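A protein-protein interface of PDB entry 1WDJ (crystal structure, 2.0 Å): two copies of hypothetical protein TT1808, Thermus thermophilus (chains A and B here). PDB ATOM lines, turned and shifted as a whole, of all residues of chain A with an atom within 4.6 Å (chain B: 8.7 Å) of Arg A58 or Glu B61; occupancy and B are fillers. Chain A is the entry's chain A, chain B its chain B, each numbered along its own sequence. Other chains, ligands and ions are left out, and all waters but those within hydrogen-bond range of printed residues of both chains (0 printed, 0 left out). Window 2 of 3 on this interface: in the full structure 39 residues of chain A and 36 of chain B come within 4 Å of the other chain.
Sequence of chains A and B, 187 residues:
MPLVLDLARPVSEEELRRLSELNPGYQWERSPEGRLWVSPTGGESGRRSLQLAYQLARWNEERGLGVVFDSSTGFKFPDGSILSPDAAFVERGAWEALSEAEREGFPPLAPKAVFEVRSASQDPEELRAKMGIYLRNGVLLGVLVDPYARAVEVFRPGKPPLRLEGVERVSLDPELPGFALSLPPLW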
ATOM      1  N   TYR A  54       8.737  19.596   0.545  1.00  0.00           N
ATOM      2  CA  TYR A  54      10.078  19.082   0.338  1.00  0.00           C
ATOM      3  C   TYR A  54      11.134  20.175   0.556  1.00  0.00           C
ATOM      4  O   TYR A  54      12.172  19.947   1.194  1.00  0.00           O
ATOM      5  CB  TYR A  54      10.198  18.518  -1.085  1.00  0.00           C
ATOM      6  CG  TYR A  54      11.617  18.452  -1.590  1.00  0.00           C
ATOM      7  CD1 TYR A  54      12.519  17.512  -1.082  1.00  0.00           C
ATOM      8  CD2 TYR A  54      12.076  19.360  -2.542  1.00  0.00           C
ATOM      9  CE1 TYR A  54      13.840  17.477  -1.504  1.00  0.00           C
ATOM     10  CE2 TYR A  54      13.397  19.338  -2.974  1.00  0.00           C
ATOM     11  CZ  TYR A  54      14.276  18.392  -2.450  1.00  0.00           C
ATOM     12  OH  TYR A  54      15.589  18.365  -2.876  1.00  0.00           O
ATOM     13  N   GLN A  55      10.888  21.359   0.006  1.00  0.00           N
ATOM     14  CA  GLN A  55      11.843  22.443   0.168  1.00  0.00           C
ATOM     15  C   GLN A  55      11.917  22.878   1.629  1.00  0.00           C
ATOM     16  O   GLN A  55      13.001  23.164   2.158  1.00  0.00           O
ATOM     17  CB  GLN A  55      11.459  23.621  -0.718  1.00  0.00           C
ATOM     18  CG  GLN A  55      11.659  23.323  -2.203  1.00  0.00           C
ATOM     19  CD  GLN A  55      11.424  24.545  -3.063  1.00  0.00           C
ATOM     20  OE1 GLN A  55      11.892  25.644  -2.744  1.00  0.00           O
ATOM     21  NE2 GLN A  55      10.705  24.361  -4.167  1.00  0.00           N
ATOM     22  N   LEU A  56      10.758  22.935   2.277  1.00  0.00           N
ATOM     23  CA  LEU A  56      10.715  23.326   3.677  1.00  0.00           C
ATOM     24  C   LEU A  56      11.483  22.268   4.497  1.00  0.00           C
ATOM     25  O   LEU A  56      12.322  22.606   5.321  1.00  0.00           O
ATOM     26  CB  LEU A  56       9.253  23.413   4.147  1.00  0.00           C
ATOM     27  CG  LEU A  56       9.051  24.025   5.541  1.00  0.00           C
ATOM     28  CD1 LEU A  56       9.655  25.439   5.552  1.00  0.00           C
ATOM     29  CD2 LEU A  56       7.559  24.056   5.900  1.00  0.00           C
ATOM     30  N   ALA A  57      11.204  20.992   4.246  1.00  0.00           N
ATOM     31  CA  ALA A  57      11.852  19.899   4.973  1.00  0.00           C
ATOM     32  C   ALA A  57      13.380  19.894   4.784  1.00  0.00           C
ATOM     33  O   ALA A  57      14.122  19.714   5.756  1.00  0.00           O
ATOM     34  CB  ALA A  57      11.260  18.560   4.530  1.00  0.00           C
ATOM     35  N   ARG A  58      13.827  20.080   3.535  1.00  0.00           N
ATOM     36  CA  ARG A  58      15.248  20.129   3.197  1.00  0.00           C
ATOM     37  C   ARG A  58      15.904  21.214   4.015  1.00  0.00           C
ATOM     38  O   ARG A  58      16.926  20.988   4.658  1.00  0.00           O
ATOM     39  CB  ARG A  58      15.444  20.442   1.714  1.00  0.00           C
ATOM     40  CG  ARG A  58      16.905  20.325   1.252  1.00  0.00           C
ATOM     41  CD  ARG A  58      17.028  20.424  -0.278  1.00  0.00           C
ATOM     42  NE  ARG A  58      16.540  21.699  -0.808  1.00  0.00           N
ATOM     43  CZ  ARG A  58      16.288  21.927  -2.097  1.00  0.00           C
ATOM     44  NH1 ARG A  58      16.480  20.961  -2.994  1.00  0.00           N
ATOM     45  NH2 ARG A  58      15.838  23.116  -2.490  1.00  0.00           N
ATOM     46  N   TRP A  59      15.310  22.403   3.991  1.00  0.00           N
ATOM     47  CA  TRP A  59      15.834  23.514   4.766  1.00  0.00           C
ATOM     48  C   TRP A  59      15.879  23.120   6.258  1.00  0.00           C
ATOM     49  O   TRP A  59      16.890  23.295   6.938  1.00  0.00           O
ATOM     50  CB  TRP A  59      14.939  24.747   4.584  1.00  0.00           C
ATOM     51  CG  TRP A  59      15.247  25.849   5.553  1.00  0.00           C
ATOM     52  CD1 TRP A  59      16.300  26.732   5.494  1.00  0.00           C
ATOM     53  CD2 TRP A  59      14.517  26.181   6.741  1.00  0.00           C
ATOM     54  NE1 TRP A  59      16.263  27.591   6.567  1.00  0.00           N
ATOM     55  CE2 TRP A  59      15.178  27.278   7.349  1.00  0.00           C
ATOM     56  CE3 TRP A  59      13.368  25.665   7.350  1.00  0.00           C
ATOM     57  CZ2 TRP A  59      14.723  27.868   8.541  1.00  0.00           C
ATOM     58  CZ3 TRP A  59      12.914  26.260   8.544  1.00  0.00           C
ATOM     59  CH2 TRP A  59      13.595  27.347   9.117  1.00  0.00           C
ATOM     60  N   ASN A  60      14.773  22.588   6.770  1.00  0.00           N
ATOM     61  CA  ASN A  60      14.723  22.212   8.179  1.00  0.00           C
ATOM     62  C   ASN A  60      15.727  21.112   8.561  1.00  0.00           C
ATOM     63  O   ASN A  60      16.292  21.130   9.661  1.00  0.00           O
ATOM     64  CB  ASN A  60      13.314  21.766   8.565  1.00  0.00           C
ATOM     65  CG  ASN A  60      13.155  21.613  10.067  1.00  0.00           C
ATOM     66  OD1 ASN A  60      13.418  22.550  10.822  1.00  0.00           O
ATOM     67  ND2 ASN A  60      12.732  20.432  10.508  1.00  0.00           N
ATOM     68  N   GLU A  61      15.949  20.158   7.663  1.00  0.00           N
ATOM     69  CA  GLU A  61      16.888  19.082   7.955  1.00  0.00           C
ATOM     70  C   GLU A  61      18.284  19.655   8.107  1.00  0.00           C
ATOM     71  O   GLU A  61      19.051  19.215   8.958  1.00  0.00           O
ATOM     72  CB  GLU A  61      16.895  18.008   6.853  1.00  0.00           C
ATOM     73  CG  GLU A  61      17.754  16.783   7.222  1.00  0.00           C
ATOM     74  CD  GLU A  61      17.810  15.696   6.138  1.00  0.00           C
ATOM     75  OE1 GLU A  61      18.281  15.992   5.014  1.00  0.00           O
ATOM     76  OE2 GLU A  61      17.394  14.543   6.417  1.00  0.00           O
ATOM     77  N   GLU A  62      18.619  20.649   7.294  1.00  0.00           N
ATOM     78  CA  GLU A  62      19.948  21.231   7.385  1.00  0.00           C
ATOM     79  C   GLU A  62      20.087  22.214   8.544  1.00  0.00           C
ATOM     80  O   GLU A  62      21.196  22.471   9.003  1.00  0.00           O
ATOM     81  CB  GLU A  62      20.351  21.887   6.051  1.00  0.00           C
ATOM     82  CG  GLU A  62      19.435  22.987   5.546  1.00  0.00           C
ATOM     83  CD  GLU A  62      19.944  23.654   4.261  1.00  0.00           C
ATOM     84  OE1 GLU A  62      20.144  22.936   3.250  1.00  0.00           O
ATOM     85  OE2 GLU A  62      20.140  24.895   4.265  1.00  0.00           O
ATOM     86  N   LEU B  50       5.533  13.411   6.300  1.00  0.00           N
ATOM     87  CA  LEU B  50       6.377  14.405   5.638  1.00  0.00           C
ATOM     88  C   LEU B  50       7.829  13.919   5.572  1.00  0.00           C
ATOM     89  O   LEU B  50       8.513  14.120   4.565  1.00  0.00           O
ATOM     90  CB  LEU B  50       6.330  15.774   6.345  1.00  0.00           C
ATOM     91  CG  LEU B  50       7.284  16.786   5.675  1.00  0.00           C
ATOM     92  CD1 LEU B  50       6.530  18.025   5.247  1.00  0.00           C
ATOM     93  CD2 LEU B  50       8.428  17.137   6.634  1.00  0.00           C
ATOM     94  N   GLN B  51       8.291  13.286   6.647  1.00  0.00           N
ATOM     95  CA  GLN B  51       9.651  12.772   6.712  1.00  0.00           C
ATOM     96  C   GLN B  51       9.839  11.727   5.607  1.00  0.00           C
ATOM     97  O   GLN B  51      10.866  11.695   4.911  1.00  0.00           O
ATOM     98  CB  GLN B  51       9.890  12.158   8.087  1.00  0.00           C
ATOM     99  CG  GLN B  51      11.325  12.149   8.535  1.00  0.00           C
ATOM    100  CD  GLN B  51      11.940  13.535   8.493  1.00  0.00           C
ATOM    101  OE1 GLN B  51      11.346  14.515   8.961  1.00  0.00           O
ATOM    102  NE2 GLN B  51      13.138  13.627   7.929  1.00  0.00           N
ATOM    103  N   ALA B  53       7.851  11.367   2.792  1.00  0.00           N
ATOM    104  CA  ALA B  53       7.683  12.050   1.516  1.00  0.00           C
ATOM    105  C   ALA B  53       8.929  12.853   1.156  1.00  0.00           C
ATOM    106  O   ALA B  53       9.359  12.870  -0.003  1.00  0.00           O
ATOM    107  CB  ALA B  53       6.439  12.965   1.560  1.00  0.00           C
ATOM    108  N   TYR B  54       9.509  13.515   2.152  1.00  0.00           N
ATOM    109  CA  TYR B  54      10.726  14.288   1.957  1.00  0.00           C
ATOM    110  C   TYR B  54      11.831  13.434   1.303  1.00  0.00           C
ATOM    111  O   TYR B  54      12.474  13.865   0.331  1.00  0.00           O
ATOM    112  CB  TYR B  54      11.212  14.835   3.305  1.00  0.00           C
ATOM    113  CG  TYR B  54      12.638  15.306   3.287  1.00  0.00           C
ATOM    114  CD1 TYR B  54      13.044  16.342   2.444  1.00  0.00           C
ATOM    115  CD2 TYR B  54      13.605  14.671   4.066  1.00  0.00           C
ATOM    116  CE1 TYR B  54      14.393  16.729   2.375  1.00  0.00           C
ATOM    117  CE2 TYR B  54      14.939  15.044   4.002  1.00  0.00           C
ATOM    118  CZ  TYR B  54      15.325  16.072   3.155  1.00  0.00           C
ATOM    119  OH  TYR B  54      16.649  16.435   3.104  1.00  0.00           O
ATOM    120  N   GLN B  55      12.053  12.224   1.823  1.00  0.00           N
ATOM    121  CA  GLN B  55      13.075  11.352   1.235  1.00  0.00           C
ATOM    122  C   GLN B  55      12.753  10.996  -0.229  1.00  0.00           C
ATOM    123  O   GLN B  55      13.602  11.111  -1.106  1.00  0.00           O
ATOM    124  CB  GLN B  55      13.233  10.081   2.072  1.00  0.00           C
ATOM    125  CG  GLN B  55      13.874  10.343   3.447  1.00  0.00           C
ATOM    126  CD  GLN B  55      14.091   9.074   4.234  1.00  0.00           C
ATOM    127  OE1 GLN B  55      14.625   8.100   3.713  1.00  0.00           O
ATOM    128  NE2 GLN B  55      13.674   9.075   5.500  1.00  0.00           N
ATOM    129  N   LEU B  56      11.519  10.584  -0.480  1.00  0.00           N
ATOM    130  CA  LEU B  56      11.078  10.205  -1.817  1.00  0.00           C
ATOM    131  C   LEU B  56      11.255  11.391  -2.742  1.00  0.00           C
ATOM    132  O   LEU B  56      11.722  11.239  -3.870  1.00  0.00           O
ATOM    133  CB  LEU B  56       9.601   9.777  -1.789  1.00  0.00           C
ATOM    134  CG  LEU B  56       8.914   9.307  -3.086  1.00  0.00           C
ATOM    135  CD1 LEU B  56       9.572   8.022  -3.610  1.00  0.00           C
ATOM    136  CD2 LEU B  56       7.417   9.050  -2.804  1.00  0.00           C
ATOM    137  N   ALA B  57      10.891  12.580  -2.268  1.00  0.00           N
ATOM    138  CA  ALA B  57      11.031  13.765  -3.115  1.00  0.00           C
ATOM    139  C   ALA B  57      12.505  14.101  -3.360  1.00  0.00           C
ATOM    140  O   ALA B  57      12.869  14.535  -4.454  1.00  0.00           O
ATOM    141  CB  ALA B  57      10.327  14.961  -2.493  1.00  0.00           C
ATOM    142  N   ARG B  58      13.343  13.913  -2.345  1.00  0.00           N
ATOM    143  CA  ARG B  58      14.766  14.209  -2.470  1.00  0.00           C
ATOM    144  C   ARG B  58      15.345  13.330  -3.573  1.00  0.00           C
ATOM    145  O   ARG B  58      16.105  13.796  -4.422  1.00  0.00           O
ATOM    146  CB  ARG B  58      15.468  13.942  -1.142  1.00  0.00           C
ATOM    147  CG  ARG B  58      16.921  14.353  -1.081  1.00  0.00           C
ATOM    148  CD  ARG B  58      17.466  14.166   0.343  1.00  0.00           C
ATOM    149  NE  ARG B  58      17.283  12.795   0.823  1.00  0.00           N
ATOM    150  CZ  ARG B  58      17.524  12.377   2.067  1.00  0.00           C
ATOM    151  NH1 ARG B  58      17.963  13.218   3.000  1.00  0.00           N
ATOM    152  NH2 ARG B  58      17.330  11.102   2.380  1.00  0.00           N
ATOM    153  N   TRP B  59      14.964  12.060  -3.560  1.00  0.00           N
ATOM    154  CA  TRP B  59      15.407  11.106  -4.566  1.00  0.00           C
ATOM    155  C   TRP B  59      14.877  11.486  -5.949  1.00  0.00           C
ATOM    156  O   TRP B  59      15.638  11.498  -6.931  1.00  0.00           O
ATOM    157  CB  TRP B  59      14.927   9.691  -4.216  1.00  0.00           C
ATOM    158  CG  TRP B  59      15.011   8.724  -5.372  1.00  0.00           C
ATOM    159  CD1 TRP B  59      16.143   8.163  -5.894  1.00  0.00           C
ATOM    160  CD2 TRP B  59      13.917   8.227  -6.161  1.00  0.00           C
ATOM    161  NE1 TRP B  59      15.827   7.342  -6.957  1.00  0.00           N
ATOM    162  CE2 TRP B  59      14.469   7.362  -7.145  1.00  0.00           C
ATOM    163  CE3 TRP B  59      12.530   8.428  -6.135  1.00  0.00           C
ATOM    164  CZ2 TRP B  59      13.676   6.696  -8.099  1.00  0.00           C
ATOM    165  CZ3 TRP B  59      11.735   7.765  -7.084  1.00  0.00           C
ATOM    166  CH2 TRP B  59      12.316   6.907  -8.053  1.00  0.00           C
ATOM    167  N   ASN B  60      13.581  11.792  -6.032  1.00  0.00           N
ATOM    168  CA  ASN B  60      12.992  12.145  -7.316  1.00  0.00           C
ATOM    169  C   ASN B  60      13.600  13.434  -7.874  1.00  0.00           C
ATOM    170  O   ASN B  60      13.742  13.576  -9.088  1.00  0.00           O
ATOM    171  CB  ASN B  60      11.462  12.270  -7.204  1.00  0.00           C
ATOM    172  CG  ASN B  60      10.775  12.334  -8.571  1.00  0.00           C
ATOM    173  OD1 ASN B  60      10.045  13.285  -8.874  1.00  0.00           O
ATOM    174  ND2 ASN B  60      11.006  11.326  -9.397  1.00  0.00           N
ATOM    175  N   GLU B  61      13.974  14.370  -7.006  1.00  0.00           N
ATOM    176  CA  GLU B  61      14.570  15.614  -7.494  1.00  0.00           C
ATOM    177  C   GLU B  61      15.855  15.348  -8.284  1.00  0.00           C
ATOM    178  O   GLU B  61      16.141  16.029  -9.279  1.00  0.00           O
ATOM    179  CB  GLU B  61      14.904  16.586  -6.345  1.00  0.00           C
ATOM    180  CG  GLU B  61      15.761  17.761  -6.827  1.00  0.00           C
ATOM    181  CD  GLU B  61      15.736  18.972  -5.901  1.00  0.00           C
ATOM    182  OE1 GLU B  61      14.625  19.407  -5.524  1.00  0.00           O
ATOM    183  OE2 GLU B  61      16.824  19.504  -5.569  1.00  0.00           O
ATOM    184  N   GLU B  62      16.635  14.363  -7.841  1.00  0.00           N
ATOM    185  CA  GLU B  62      17.885  14.076  -8.530  1.00  0.00           C
ATOM    186  C   GLU B  62      17.713  13.187  -9.750  1.00  0.00           C
ATOM    187  O   GLU B  62      18.460  13.312 -10.706  1.00  0.00           O
ATOM    188  CB  GLU B  62      18.902  13.429  -7.574  1.00  0.00           C
ATOM    189  CG  GLU B  62      19.365  14.317  -6.427  1.00  0.00           C
ATOM    190  CD  GLU B  62      19.849  15.697  -6.871  1.00  0.00           C
ATOM    191  OE1 GLU B  62      20.480  15.813  -7.942  1.00  0.00           O
ATOM    192  OE2 GLU B  62      19.614  16.674  -6.130  1.00  0.00           O
ATOM    193  N   ARG B  63      16.725  12.293  -9.714  1.00  0.00           N
ATOM    194  CA  ARG B  63      16.513  11.362 -10.809  1.00  0.00           C
ATOM    195  C   ARG B  63      15.383  11.714 -11.798  1.00  0.00           C
ATOM    196  O   ARG B  63      15.456  11.351 -12.983  1.00  0.00           O
ATOM    197  CB  ARG B  63      16.308   9.961 -10.217  1.00  0.00           C
ATOM    198  CG  ARG B  63      17.497   9.478  -9.368  1.00  0.00           C
ATOM    199  CD  ARG B  63      18.755   9.380 -10.240  1.00  0.00           C
ATOM    200  NE  ARG B  63      18.589   8.377 -11.292  1.00  0.00           N
ATOM    201  CZ  ARG B  63      18.831   7.078 -11.127  1.00  0.00           C
ATOM    202  NH1 ARG B  63      19.275   6.614  -9.957  1.00  0.00           N
ATOM    203  NH2 ARG B  63      18.575   6.235 -12.117  1.00  0.00           N
ATOM    204  N   GLY B  64      14.345  12.397 -11.318  1.00  0.00           N
ATOM    205  CA  GLY B  64      13.251  12.793 -12.192  1.00  0.00           C
ATOM    206  C   GLY B  64      12.604  11.709 -13.049  1.00  0.00           C
ATOM    207  O   GLY B  64      12.190  11.985 -14.176  1.00  0.00           O
ATOM    208  N   LEU B  65      12.490  10.490 -12.521  1.00  0.00           N
ATOM    209  CA  LEU B  65      11.883   9.376 -13.252  1.00  0.00           C
ATOM    210  C   LEU B  65      10.350   9.429 -13.202  1.00  0.00           C
ATOM    211  O   LEU B  65       9.654   8.740 -13.962  1.00  0.00           O
ATOM    212  CB  LEU B  65      12.376   8.058 -12.666  1.00  0.00           C
ATOM    213  CG  LEU B  65      13.904   7.904 -12.745  1.00  0.00           C
ATOM    214  CD1 LEU B  65      14.310   6.656 -11.988  1.00  0.00           C
ATOM    215  CD2 LEU B  65      14.351   7.816 -14.219  1.00  0.00           C
ATOM    216  N   GLY B  66       9.825  10.259 -12.304  1.00  0.00           N
ATOM    217  CA  GLY B  66       8.391  10.374 -12.206  1.00  0.00           C
ATOM    218  C   GLY B  66       7.943  11.610 -11.462  1.00  0.00           C
ATOM    219  O   GLY B  66       8.640  12.623 -11.391  1.00  0.00           O
ATOM    220  N   VAL B  67       6.756  11.511 -10.893  1.00  0.00           N
ATOM    221  CA  VAL B  67       6.171  12.601 -10.147  1.00  0.00           C
ATOM    222  C   VAL B  67       5.799  12.050  -8.768  1.00  0.00           C
ATOM    223  O   VAL B  67       5.233  10.946  -8.656  1.00  0.00           O
ATOM    224  CB  VAL B  67       4.901  13.112 -10.872  1.00  0.00           C
ATOM    225  CG1 VAL B  67       4.269  14.268 -10.085  1.00  0.00           C
ATOM    226  CG2 VAL B  67       5.266  13.563 -12.292  1.00  0.00           C
ATOM    227  N   VAL B  68       6.123  12.807  -7.726  1.00  0.00           N
ATOM    228  CA  VAL B  68       5.806  12.375  -6.372  1.00  0.00           C
ATOM    229  C   VAL B  68       4.701  13.265  -5.769  1.00  0.00           C
ATOM    230  O   VAL B  68       4.672  14.478  -5.974  1.00  0.00           O
ATOM    231  CB  VAL B  68       7.075  12.382  -5.490  1.00  0.00           C
ATOM    232  CG1 VAL B  68       6.719  11.996  -4.069  1.00  0.00           C
ATOM    233  CG2 VAL B  68       8.089  11.389  -6.050  1.00  0.00           C
ATOM    234  N   PHE B  89       4.389   7.701  -5.958  1.00  0.00           N
ATOM    235  CA  PHE B  89       5.269   7.969  -7.066  1.00  0.00           C
ATOM    236  C   PHE B  89       4.610   7.431  -8.325  1.00  0.00           C
ATOM    237  O   PHE B  89       4.221   6.261  -8.387  1.00  0.00           O
ATOM    238  CB  PHE B  89       6.613   7.255  -6.891  1.00  0.00           C
ATOM    239  CG  PHE B  89       7.445   7.238  -8.148  1.00  0.00           C
ATOM    240  CD1 PHE B  89       8.318   8.280  -8.432  1.00  0.00           C
ATOM    241  CD2 PHE B  89       7.345   6.181  -9.051  1.00  0.00           C
ATOM    242  CE1 PHE B  89       9.095   8.284  -9.600  1.00  0.00           C
ATOM    243  CE2 PHE B  89       8.121   6.168 -10.235  1.00  0.00           C
ATOM    244  CZ  PHE B  89       8.999   7.225 -10.505  1.00  0.00           C
ATOM    245  N   ARG B  92       6.986   8.696 -14.959  1.00  0.00           N
ATOM    246  CA  ARG B  92       6.870   9.793 -15.899  1.00  0.00           C
ATOM    247  C   ARG B  92       5.940   9.484 -17.071  1.00  0.00           C
ATOM    248  O   ARG B  92       5.068  10.288 -17.401  1.00  0.00           O
ATOM    249  CB  ARG B  92       8.253  10.156 -16.444  1.00  0.00           C
ATOM    250  CG  ARG B  92       8.229  11.213 -17.537  1.00  0.00           C
ATOM    251  CD  ARG B  92       9.622  11.774 -17.718  1.00  0.00           C
ATOM    252  NE  ARG B  92      10.067  12.353 -16.466  1.00  0.00           N
ATOM    253  CZ  ARG B  92       9.490  13.399 -15.887  1.00  0.00           C
ATOM    254  NH1 ARG B  92       8.448  13.992 -16.457  1.00  0.00           N
ATOM    255  NH2 ARG B  92       9.935  13.832 -14.722  1.00  0.00           N
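OE1 of Glu A61 is in salt-bridge range of NH1 of Arg B58 (3.4 Å). The side-chain hydroxyl (OH) of Tyr A54 sits close to the side-chain carboxylate (OE1) of Glu B61 (3.0 Å). The guanidinium group (NH1) of Arg A58 is in salt-bridge range of the side-chain carboxylate (OE2) of Glu B61 (3.0 Å). OE1 of Glu A61 sits at hydrogen-bond distance from OH of Tyr B54.
OH of Tyr A54 is in hydrogen-bond range of NH1 of Arg A58 (2.7 Å). NH1 of Arg B58 lies within hydrogen-bond range of OH of Tyr B54, 3.5 Å away.
CD1 of Tyr B54 touches CD1 of Tyr A54, 3.8 Å away. CB of Ala B57 touches CD1 of Tyr A54, at 3.6 Å. Tyr A54 touches Arg B58 (CE1 to CA, 3.5 Å). Ala A57 touches Leu B50 (CB to CD2, 3.8 Å). Ala A57 touches Tyr B54 (CB to CD1, 3.5 Å). N of Arg A58 touches CE1 of Tyr B54, at 3.6 Å.
Of the printed residues of chain B, Tyr A54 touches Tyr B54, Ala B57, Arg B58 and Glu B61. Ala A57 touches two residues of chain B. Of chain B, only Tyr B54 (3.6 Å) and Glu B61 (3.0 Å) come within 4 Å of Arg A58. Of the printed residues of chain B, Glu A61 touches Tyr B54 and Arg B58. Of the printed residues of chain A, Leu B50 touches Ala A57. Ala B53 touches none of the printed residues of chain A. Of the printed residues of chain A, Tyr B54 touches Tyr A54, Ala A57, Arg A58 and Glu A61. Of the printed residues of chain A, Arg B58 touches Tyr A54 and Glu A61. Glu B61 touches just these residues of chain A: Tyr A54 and Arg A58. Gly B66 touches none of the printed residues of chain A.
Hydrophobic or aromatic side chains of chain B that line the printed part of chain A: Leu B50, Tyr B54 and Ala B57. Hydrophobic or aromatic side chains of chain A within 4 Å of the printed part of chain B: Tyr A54 and Ala A57. Among the printed residues, 10 pairs touch across the chains. Among the printed residues, Asp or Glu carboxylates within 4 Å of a Lys or Arg side-chain nitrogen of the other chain: Arg A58 with Glu B61 and Glu A61 with Arg B58.
Tyr A54 touches its own counterpart, Tyr B54. Tyr A54 touches Ala B57, and with the chains exchanged Ala A57 touches Tyr B54. Tyr A54 touches Arg B58, and with the chains exchanged Arg A58 touches Tyr B54. Tyr A54 touches Glu B61, and with the chains exchanged Glu A61 touches Tyr B54. Positions printed for both chains: 54, 55, 56, 57, 58, 59, 60, 61 and 62. Of the 10 pairs that touch across the chains among the printed residues, 9 have their exchanged pair printed and touching as well.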
